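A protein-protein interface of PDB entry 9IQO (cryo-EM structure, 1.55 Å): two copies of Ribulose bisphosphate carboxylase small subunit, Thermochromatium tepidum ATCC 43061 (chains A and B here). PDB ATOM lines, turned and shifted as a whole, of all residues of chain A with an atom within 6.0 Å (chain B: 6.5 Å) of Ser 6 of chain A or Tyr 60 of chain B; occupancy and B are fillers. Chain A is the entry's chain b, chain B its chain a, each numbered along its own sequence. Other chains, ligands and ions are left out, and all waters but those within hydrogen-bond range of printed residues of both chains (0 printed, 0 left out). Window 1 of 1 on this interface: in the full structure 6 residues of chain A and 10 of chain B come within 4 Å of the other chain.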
ATOM      1  N   ASP A   3      11.091  26.887 -11.984  1.00  0.00           N
ATOM      2  CA  ASP A   3      10.488  25.569 -12.113  1.00  0.00           C
ATOM      3  C   ASP A   3      11.453  24.605 -12.788  1.00  0.00           C
ATOM      4  O   ASP A   3      12.254  24.998 -13.639  1.00  0.00           O
ATOM      5  CB  ASP A   3       9.194  25.666 -12.916  1.00  0.00           C
ATOM      6  CG  ASP A   3       8.127  24.727 -12.409  1.00  0.00           C
ATOM      7  OD1 ASP A   3       7.983  24.594 -11.178  1.00  0.00           O
ATOM      8  OD2 ASP A   3       7.431  24.123 -13.249  1.00  0.00           O
ATOM      9  N   TYR A   4      11.364  23.327 -12.414  1.00  0.00           N
ATOM     10  CA  TYR A   4      12.341  22.357 -12.890  1.00  0.00           C
ATOM     11  C   TYR A   4      12.201  22.045 -14.376  1.00  0.00           C
ATOM     12  O   TYR A   4      13.199  21.694 -15.014  1.00  0.00           O
ATOM     13  CB  TYR A   4      12.255  21.066 -12.084  1.00  0.00           C
ATOM     14  CG  TYR A   4      13.225  20.034 -12.588  1.00  0.00           C
ATOM     15  CD1 TYR A   4      14.580  20.309 -12.644  1.00  0.00           C
ATOM     16  CD2 TYR A   4      12.787  18.803 -13.046  1.00  0.00           C
ATOM     17  CE1 TYR A   4      15.471  19.386 -13.123  1.00  0.00           C
ATOM     18  CE2 TYR A   4      13.674  17.868 -13.524  1.00  0.00           C
ATOM     19  CZ  TYR A   4      15.015  18.164 -13.561  1.00  0.00           C
ATOM     20  OH  TYR A   4      15.907  17.238 -14.039  1.00  0.00           O
ATOM     21  N   ASN A   5      11.006  22.182 -14.948  1.00  0.00           N
ATOM     22  CA  ASN A   5      10.772  21.956 -16.376  1.00  0.00           C
ATOM     23  C   ASN A   5      11.084  20.506 -16.765  1.00  0.00           C
ATOM     24  O   ASN A   5      12.032  20.199 -17.488  1.00  0.00           O
ATOM     25  CB  ASN A   5      11.574  22.943 -17.233  1.00  0.00           C
ATOM     26  CG  ASN A   5      11.327  22.759 -18.716  1.00  0.00           C
ATOM     27  OD1 ASN A   5      10.206  22.927 -19.194  1.00  0.00           O
ATOM     28  ND2 ASN A   5      12.372  22.401 -19.450  1.00  0.00           N
ATOM     29  N   SER A   6      10.259  19.617 -16.226  1.00  0.00           N
ATOM     30  CA  SER A   6      10.205  18.232 -16.661  1.00  0.00           C
ATOM     31  C   SER A   6       8.749  17.801 -16.605  1.00  0.00           C
ATOM     32  O   SER A   6       8.044  18.131 -15.651  1.00  0.00           O
ATOM     33  CB  SER A   6      11.075  17.327 -15.784  1.00  0.00           C
ATOM     34  OG  SER A   6      10.940  15.969 -16.159  1.00  0.00           O
ATOM     35  N   SER A   7       8.299  17.080 -17.626  1.00  0.00           N
ATOM     36  CA  SER A   7       6.894  16.702 -17.674  1.00  0.00           C
ATOM     37  C   SER A   7       6.735  15.438 -18.502  1.00  0.00           C
ATOM     38  O   SER A   7       7.614  15.066 -19.280  1.00  0.00           O
ATOM     39  CB  SER A   7       6.032  17.830 -18.245  1.00  0.00           C
ATOM     40  OG  SER A   7       6.185  17.924 -19.646  1.00  0.00           O
ATOM     41  N   LEU A   8       5.584  14.787 -18.324  1.00  0.00           N
ATOM     42  CA  LEU A   8       5.297  13.567 -19.068  1.00  0.00           C
ATOM     43  C   LEU A   8       5.138  13.838 -20.558  1.00  0.00           C
ATOM     44  O   LEU A   8       5.502  12.993 -21.379  1.00  0.00           O
ATOM     45  CB  LEU A   8       4.039  12.896 -18.519  1.00  0.00           C
ATOM     46  CG  LEU A   8       4.087  12.416 -17.067  1.00  0.00           C
ATOM     47  CD1 LEU A   8       2.700  12.418 -16.446  1.00  0.00           C
ATOM     48  CD2 LEU A   8       4.711  11.035 -16.974  1.00  0.00           C
ATOM     49  N   GLU A   9       4.594  14.995 -20.927  1.00  0.00           N
ATOM     50  CA  GLU A   9       4.362  15.300 -22.333  1.00  0.00           C
ATOM     51  C   GLU A   9       5.584  15.869 -23.039  1.00  0.00           C
ATOM     52  O   GLU A   9       5.712  15.709 -24.257  1.00  0.00           O
ATOM     53  CB  GLU A   9       3.189  16.272 -22.475  1.00  0.00           C
ATOM     54  CG  GLU A   9       1.847  15.675 -22.093  1.00  0.00           C
ATOM     55  CD  GLU A   9       1.756  14.188 -22.383  1.00  0.00           C
ATOM     56  OE1 GLU A   9       1.877  13.799 -23.564  1.00  0.00           O
ATOM     57  OE2 GLU A   9       1.564  13.406 -21.429  1.00  0.00           O
ATOM     58  N   ASP A  10       6.485  16.525 -22.314  1.00  0.00           N
ATOM     59  CA  ASP A  10       7.687  17.082 -22.925  1.00  0.00           C
ATOM     60  C   ASP A  10       8.664  15.947 -23.211  1.00  0.00           C
ATOM     61  O   ASP A  10       9.209  15.338 -22.286  1.00  0.00           O
ATOM     62  CB  ASP A  10       8.306  18.127 -22.001  1.00  0.00           C
ATOM     63  CG  ASP A  10       9.565  18.754 -22.575  1.00  0.00           C
ATOM     64  OD1 ASP A  10       9.892  18.500 -23.753  1.00  0.00           O
ATOM     65  OD2 ASP A  10      10.235  19.505 -21.837  1.00  0.00           O
ATOM     66  N   SER A  13      12.114  15.673 -21.657  1.00  0.00           N
ATOM     67  CA  SER A  13      12.265  15.255 -20.272  1.00  0.00           C
ATOM     68  C   SER A  13      12.870  13.864 -20.153  1.00  0.00           C
ATOM     69  O   SER A  13      13.418  13.532 -19.098  1.00  0.00           O
ATOM     70  CB  SER A  13      10.914  15.295 -19.564  1.00  0.00           C
ATOM     71  OG  SER A  13      10.334  16.582 -19.653  1.00  0.00           O
ATOM     72  N   ILE B  46       0.895  26.057  -5.685  1.00  0.00           N
ATOM     73  CA  ILE B  46       0.369  25.981  -7.039  1.00  0.00           C
ATOM     74  C   ILE B  46       0.816  24.660  -7.641  1.00  0.00           C
ATOM     75  O   ILE B  46       2.009  24.339  -7.621  1.00  0.00           O
ATOM     76  CB  ILE B  46       0.852  27.160  -7.901  1.00  0.00           C
ATOM     77  CG1 ILE B  46       0.433  28.488  -7.273  1.00  0.00           C
ATOM     78  CG2 ILE B  46       0.331  27.034  -9.318  1.00  0.00           C
ATOM     79  CD1 ILE B  46      -1.054  28.640  -7.107  1.00  0.00           C
ATOM     80  N   GLU B  47      -0.133  23.892  -8.157  1.00  0.00           N
ATOM     81  CA  GLU B  47       0.209  22.737  -8.969  1.00  0.00           C
ATOM     82  C   GLU B  47      -0.440  22.856 -10.336  1.00  0.00           C
ATOM     83  O   GLU B  47      -1.326  23.675 -10.562  1.00  0.00           O
ATOM     84  CB  GLU B  47      -0.187  21.409  -8.309  1.00  0.00           C
ATOM     85  CG  GLU B  47       0.347  21.198  -6.909  1.00  0.00           C
ATOM     86  CD  GLU B  47      -0.182  19.925  -6.274  1.00  0.00           C
ATOM     87  OE1 GLU B  47      -1.109  19.314  -6.843  1.00  0.00           O
ATOM     88  OE2 GLU B  47       0.322  19.538  -5.201  1.00  0.00           O
ATOM     89  N   HIS B  48       0.034  22.035 -11.260  1.00  0.00           N
ATOM     90  CA  HIS B  48      -0.513  22.046 -12.604  1.00  0.00           C
ATOM     91  C   HIS B  48      -0.271  20.689 -13.234  1.00  0.00           C
ATOM     92  O   HIS B  48       0.619  19.948 -12.815  1.00  0.00           O
ATOM     93  CB  HIS B  48       0.109  23.160 -13.449  1.00  0.00           C
ATOM     94  CG  HIS B  48       1.555  22.941 -13.759  1.00  0.00           C
ATOM     95  ND1 HIS B  48       1.988  22.410 -14.953  1.00  0.00           N
ATOM     96  CD2 HIS B  48       2.667  23.168 -13.023  1.00  0.00           C
ATOM     97  CE1 HIS B  48       3.304  22.329 -14.944  1.00  0.00           C
ATOM     98  NE2 HIS B  48       3.742  22.782 -13.785  1.00  0.00           N
ATOM     99  N   THR B  49      -1.078  20.369 -14.236  1.00  0.00           N
ATOM    100  CA  THR B  49      -0.915  19.114 -14.949  1.00  0.00           C
ATOM    101  C   THR B  49      -1.598  19.223 -16.298  1.00  0.00           C
ATOM    102  O   THR B  49      -2.478  20.059 -16.507  1.00  0.00           O
ATOM    103  CB  THR B  49      -1.485  17.932 -14.157  1.00  0.00           C
ATOM    104  OG1 THR B  49      -0.956  16.710 -14.682  1.00  0.00           O
ATOM    105  CG2 THR B  49      -2.997  17.904 -14.250  1.00  0.00           C
ATOM    106  N   GLU B  50      -1.175  18.363 -17.212  1.00  0.00           N
ATOM    107  CA  GLU B  50      -1.881  18.236 -18.470  1.00  0.00           C
ATOM    108  C   GLU B  50      -3.277  17.684 -18.201  1.00  0.00           C
ATOM    109  O   GLU B  50      -3.446  16.833 -17.322  1.00  0.00           O
ATOM    110  CB  GLU B  50      -1.115  17.315 -19.417  1.00  0.00           C
ATOM    111  CG  GLU B  50       0.291  17.794 -19.712  1.00  0.00           C
ATOM    112  CD  GLU B  50       1.339  17.058 -18.898  1.00  0.00           C
ATOM    113  OE1 GLU B  50       2.542  17.219 -19.186  1.00  0.00           O
ATOM    114  OE2 GLU B  50       0.961  16.315 -17.969  1.00  0.00           O
ATOM    115  N   HIS B  53      -3.922  13.991 -17.615  1.00  0.00           N
ATOM    116  CA  HIS B  53      -3.354  13.387 -16.409  1.00  0.00           C
ATOM    117  C   HIS B  53      -3.945  13.989 -15.141  1.00  0.00           C
ATOM    118  O   HIS B  53      -3.362  13.887 -14.067  1.00  0.00           O
ATOM    119  CB  HIS B  53      -1.839  13.535 -16.420  1.00  0.00           C
ATOM    120  CG  HIS B  53      -1.182  12.911 -17.610  1.00  0.00           C
ATOM    121  ND1 HIS B  53      -1.526  11.663 -18.079  1.00  0.00           N
ATOM    122  CD2 HIS B  53      -0.216  13.371 -18.437  1.00  0.00           C
ATOM    123  CE1 HIS B  53      -0.790  11.374 -19.137  1.00  0.00           C
ATOM    124  NE2 HIS B  53       0.012  12.396 -19.377  1.00  0.00           N
ATOM    125  N   TYR B  58      -0.574  12.917  -8.021  1.00  0.00           N
ATOM    126  CA  TYR B  58       0.468  13.931  -7.983  1.00  0.00           C
ATOM    127  C   TYR B  58       0.426  14.737  -9.270  1.00  0.00           C
ATOM    128  O   TYR B  58       0.624  14.188 -10.357  1.00  0.00           O
ATOM    129  CB  TYR B  58       1.838  13.286  -7.789  1.00  0.00           C
ATOM    130  CG  TYR B  58       1.980  12.634  -6.441  1.00  0.00           C
ATOM    131  CD1 TYR B  58       1.768  13.359  -5.283  1.00  0.00           C
ATOM    132  CD2 TYR B  58       2.299  11.291  -6.324  1.00  0.00           C
ATOM    133  CE1 TYR B  58       1.884  12.777  -4.051  1.00  0.00           C
ATOM    134  CE2 TYR B  58       2.417  10.698  -5.088  1.00  0.00           C
ATOM    135  CZ  TYR B  58       2.206  11.448  -3.956  1.00  0.00           C
ATOM    136  OH  TYR B  58       2.317  10.877  -2.717  1.00  0.00           O
ATOM    137  N   TRP B  59       0.154  16.026  -9.141  1.00  0.00           N
ATOM    138  CA  TRP B  59       0.326  16.960 -10.235  1.00  0.00           C
ATOM    139  C   TRP B  59       1.751  17.498 -10.184  1.00  0.00           C
ATOM    140  O   TRP B  59       2.519  17.190  -9.274  1.00  0.00           O
ATOM    141  CB  TRP B  59      -0.698  18.086 -10.142  1.00  0.00           C
ATOM    142  CG  TRP B  59      -2.090  17.674 -10.459  1.00  0.00           C
ATOM    143  CD1 TRP B  59      -2.606  16.416 -10.414  1.00  0.00           C
ATOM    144  CD2 TRP B  59      -3.157  18.531 -10.867  1.00  0.00           C
ATOM    145  NE1 TRP B  59      -3.930  16.434 -10.773  1.00  0.00           N
ATOM    146  CE2 TRP B  59      -4.292  17.724 -11.056  1.00  0.00           C
ATOM    147  CE3 TRP B  59      -3.261  19.904 -11.097  1.00  0.00           C
ATOM    148  CZ2 TRP B  59      -5.515  18.244 -11.461  1.00  0.00           C
ATOM    149  CZ3 TRP B  59      -4.473  20.416 -11.497  1.00  0.00           C
ATOM    150  CH2 TRP B  59      -5.585  19.590 -11.676  1.00  0.00           C
ATOM    151  N   TYR B  60       2.120  18.308 -11.168  1.00  0.00           N
ATOM    152  CA  TYR B  60       3.412  18.974 -11.125  1.00  0.00           C
ATOM    153  C   TYR B  60       3.351  20.119 -10.131  1.00  0.00           C
ATOM    154  O   TYR B  60       2.451  20.958 -10.201  1.00  0.00           O
ATOM    155  CB  TYR B  60       3.807  19.509 -12.498  1.00  0.00           C
ATOM    156  CG  TYR B  60       3.798  18.486 -13.599  1.00  0.00           C
ATOM    157  CD1 TYR B  60       4.639  17.385 -13.559  1.00  0.00           C
ATOM    158  CD2 TYR B  60       2.963  18.632 -14.692  1.00  0.00           C
ATOM    159  CE1 TYR B  60       4.634  16.454 -14.569  1.00  0.00           C
ATOM    160  CE2 TYR B  60       2.952  17.709 -15.705  1.00  0.00           C
ATOM    161  CZ  TYR B  60       3.787  16.622 -15.641  1.00  0.00           C
ATOM    162  OH  TYR B  60       3.774  15.700 -16.658  1.00  0.00           O
ATOM    163  N   MET B  61       4.300  20.158  -9.207  1.00  0.00           N
ATOM    164  CA  MET B  61       4.422  21.311  -8.331  1.00  0.00           C
ATOM    165  C   MET B  61       5.024  22.470  -9.110  1.00  0.00           C
ATOM    166  O   MET B  61       6.031  22.305  -9.804  1.00  0.00           O
ATOM    167  CB  MET B  61       5.288  20.996  -7.115  1.00  0.00           C
ATOM    168  CG  MET B  61       5.398  22.132  -6.124  1.00  0.00           C
ATOM    169  SD  MET B  61       6.334  21.672  -4.657  1.00  0.00           S
ATOM    170  CE  MET B  61       5.112  20.731  -3.763  1.00  0.00           C
ATOM    171  N   TRP B  62       4.401  23.635  -9.007  1.00  0.00           N
ATOM    172  CA  TRP B  62       4.970  24.861  -9.549  1.00  0.00           C
ATOM    173  C   TRP B  62       5.890  25.445  -8.486  1.00  0.00           C
ATOM    174  O   TRP B  62       5.422  26.052  -7.520  1.00  0.00           O
ATOM    175  CB  TRP B  62       3.877  25.847  -9.941  1.00  0.00           C
ATOM    176  CG  TRP B  62       4.405  27.173 -10.375  1.00  0.00           C
ATOM    177  CD1 TRP B  62       4.407  28.329  -9.657  1.00  0.00           C
ATOM    178  CD2 TRP B  62       5.014  27.483 -11.632  1.00  0.00           C
ATOM    179  NE1 TRP B  62       4.976  29.340 -10.387  1.00  0.00           N
ATOM    180  CE2 TRP B  62       5.357  28.846 -11.606  1.00  0.00           C
ATOM    181  CE3 TRP B  62       5.300  26.739 -12.779  1.00  0.00           C
ATOM    182  CZ2 TRP B  62       5.972  29.480 -12.678  1.00  0.00           C
ATOM    183  CZ3 TRP B  62       5.910  27.371 -13.841  1.00  0.00           C
ATOM    184  CH2 TRP B  62       6.239  28.727 -13.783  1.00  0.00           C
ATOM    185  N   CYS B  82       2.510  30.507 -13.389  1.00  0.00           N
ATOM    186  CA  CYS B  82       2.347  29.099 -13.738  1.00  0.00           C
ATOM    187  C   CYS B  82       1.412  28.939 -14.926  1.00  0.00           C
ATOM    188  O   CYS B  82       1.671  28.133 -15.826  1.00  0.00           O
ATOM    189  CB  CYS B  82       1.823  28.307 -12.543  1.00  0.00           C
ATOM    190  SG  CYS B  82       1.525  26.562 -12.909  1.00  0.00           S
ATOM    191  N   ASN B  89      -2.361  23.686 -19.423  1.00  0.00           N
ATOM    192  CA  ASN B  89      -2.486  22.848 -18.245  1.00  0.00           C
ATOM    193  C   ASN B  89      -3.549  23.389 -17.300  1.00  0.00           C
ATOM    194  O   ASN B  89      -3.789  24.595 -17.230  1.00  0.00           O
ATOM    195  CB  ASN B  89      -1.150  22.750 -17.508  1.00  0.00           C
ATOM    196  CG  ASN B  89      -0.188  21.803 -18.179  1.00  0.00           C
ATOM    197  OD1 ASN B  89      -0.470  21.273 -19.249  1.00  0.00           O
ATOM    198  ND2 ASN B  89       0.955  21.579 -17.551  1.00  0.00           N
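O of Met 61 of chain B sits close to OD1 of Asp 3 of chain A (3.3 Å).
The side-chain hydroxyl (OH) of Tyr 60 of chain B lies within hydrogen-bond range of the backbone NH (N) of Leu 8 of chain A (2.6 Å).
The backbone NH (N) of Glu 9 of chain A lies close to the side-chain carboxylate (OE1) of Glu 50 of chain B (3.5 Å).
OE2 of Glu 9 of chain A is in hydrogen-bond range of NE2 of His 53 of chain B (2.8 Å).
The backbone NH of Trp 62 of chain B sits at hydrogen-bond distance from the backbone carbonyl oxygen of Ile 46 of chain B (2.9 Å).
The side-chain hydroxyl (OG) of Ser 7 of chain A is in hydrogen-bond range of the backbone NH (N) of Asp 10 of chain A, 3.0 Å away.
The backbone carbonyl oxygen (O) of His 48 of chain B sits at hydrogen-bond distance from the backbone NH (N) of Tyr 60 of chain B.
A ring nitrogen (ND1) of His 48 of chain B sits at hydrogen-bond distance from the side-chain amide nitrogen (ND2) of Asn 89 of chain B (2.9 Å).
OE2 of Glu 50 of chain B sits at hydrogen-bond distance from OH of Tyr 60 of chain B (3.2 Å).
The backbone NH (N) of Ser 7 of chain A sits at hydrogen-bond distance from the side-chain hydroxyl (OG) of Ser 13 of chain A (2.9 Å).
Among the printed residues, pairs that only touch across the chains: Asp 3 of chain A with His 48 of chain B (3.96 Å), Asp 3 of chain A with Trp 62 of chain B (3.4 Å), Ser 6 of chain A with Tyr 60 of chain B (3.95 Å), Ser 7 of chain A with Glu 50 of chain B (3.7 Å), Ser 7 of chain A with Tyr 60 of chain B (3.4 Å), Leu 8 of chain A with Glu 50 of chain B (3.99 Å) and Leu 8 of chain A with His 53 of chain B (3.7 Å).
Of chain B, only Tyr 60 (3.95 Å) comes within 4 Å of Ser 6 of chain A.
Tyr 60 of chain B touches just these residues of chain A: Ser 6, Ser 7 and Leu 8.
Of the printed residues of chain A, Glu 50 of chain B touches Ser 7 (3.7 Å), Leu 8 (3.99 Å) and Glu 9 (3.4 Å).
Of the printed residues of chain B, Glu 9 of chain A touches Glu 50 and His 53.
Of the printed residues of chain B, Asp 3 of chain A touches His 48, Met 61 and Trp 62.
Of the printed residues of chain B, Ser 7 of chain A touches Glu 50 and Tyr 60.
Glu 47 of chain B touches none of the printed residues of chain A.
Tyr 4 of chain A touches none of the printed residues of chain B.
The nearest residue of chain A that does not touch Tyr 60 of chain B is Glu 9 of chain A (4.4 Å).
Of the 9 printed residues of chain A, 5 touch a printed residue of chain B.
Printed residues of chain A that touch a printed residue of chain B: Asp 3, Ser 6, Ser 7, Leu 8 and Glu 9.
Hydrophobic or aromatic side chains of chain A that line the printed part of chain B: Leu 8.
Along chain A the printed residues that touch a printed residue of chain B span positions 3 to 9.
Among the printed residues, no Asp or Glu carboxylate lies within 4 Å of a Lys or Arg side-chain nitrogen of the other chain.
No position is printed for both chains.
Of the 11 pairs that touch across the chains among the printed residues, none has its exchanged pair printed and touching as well.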
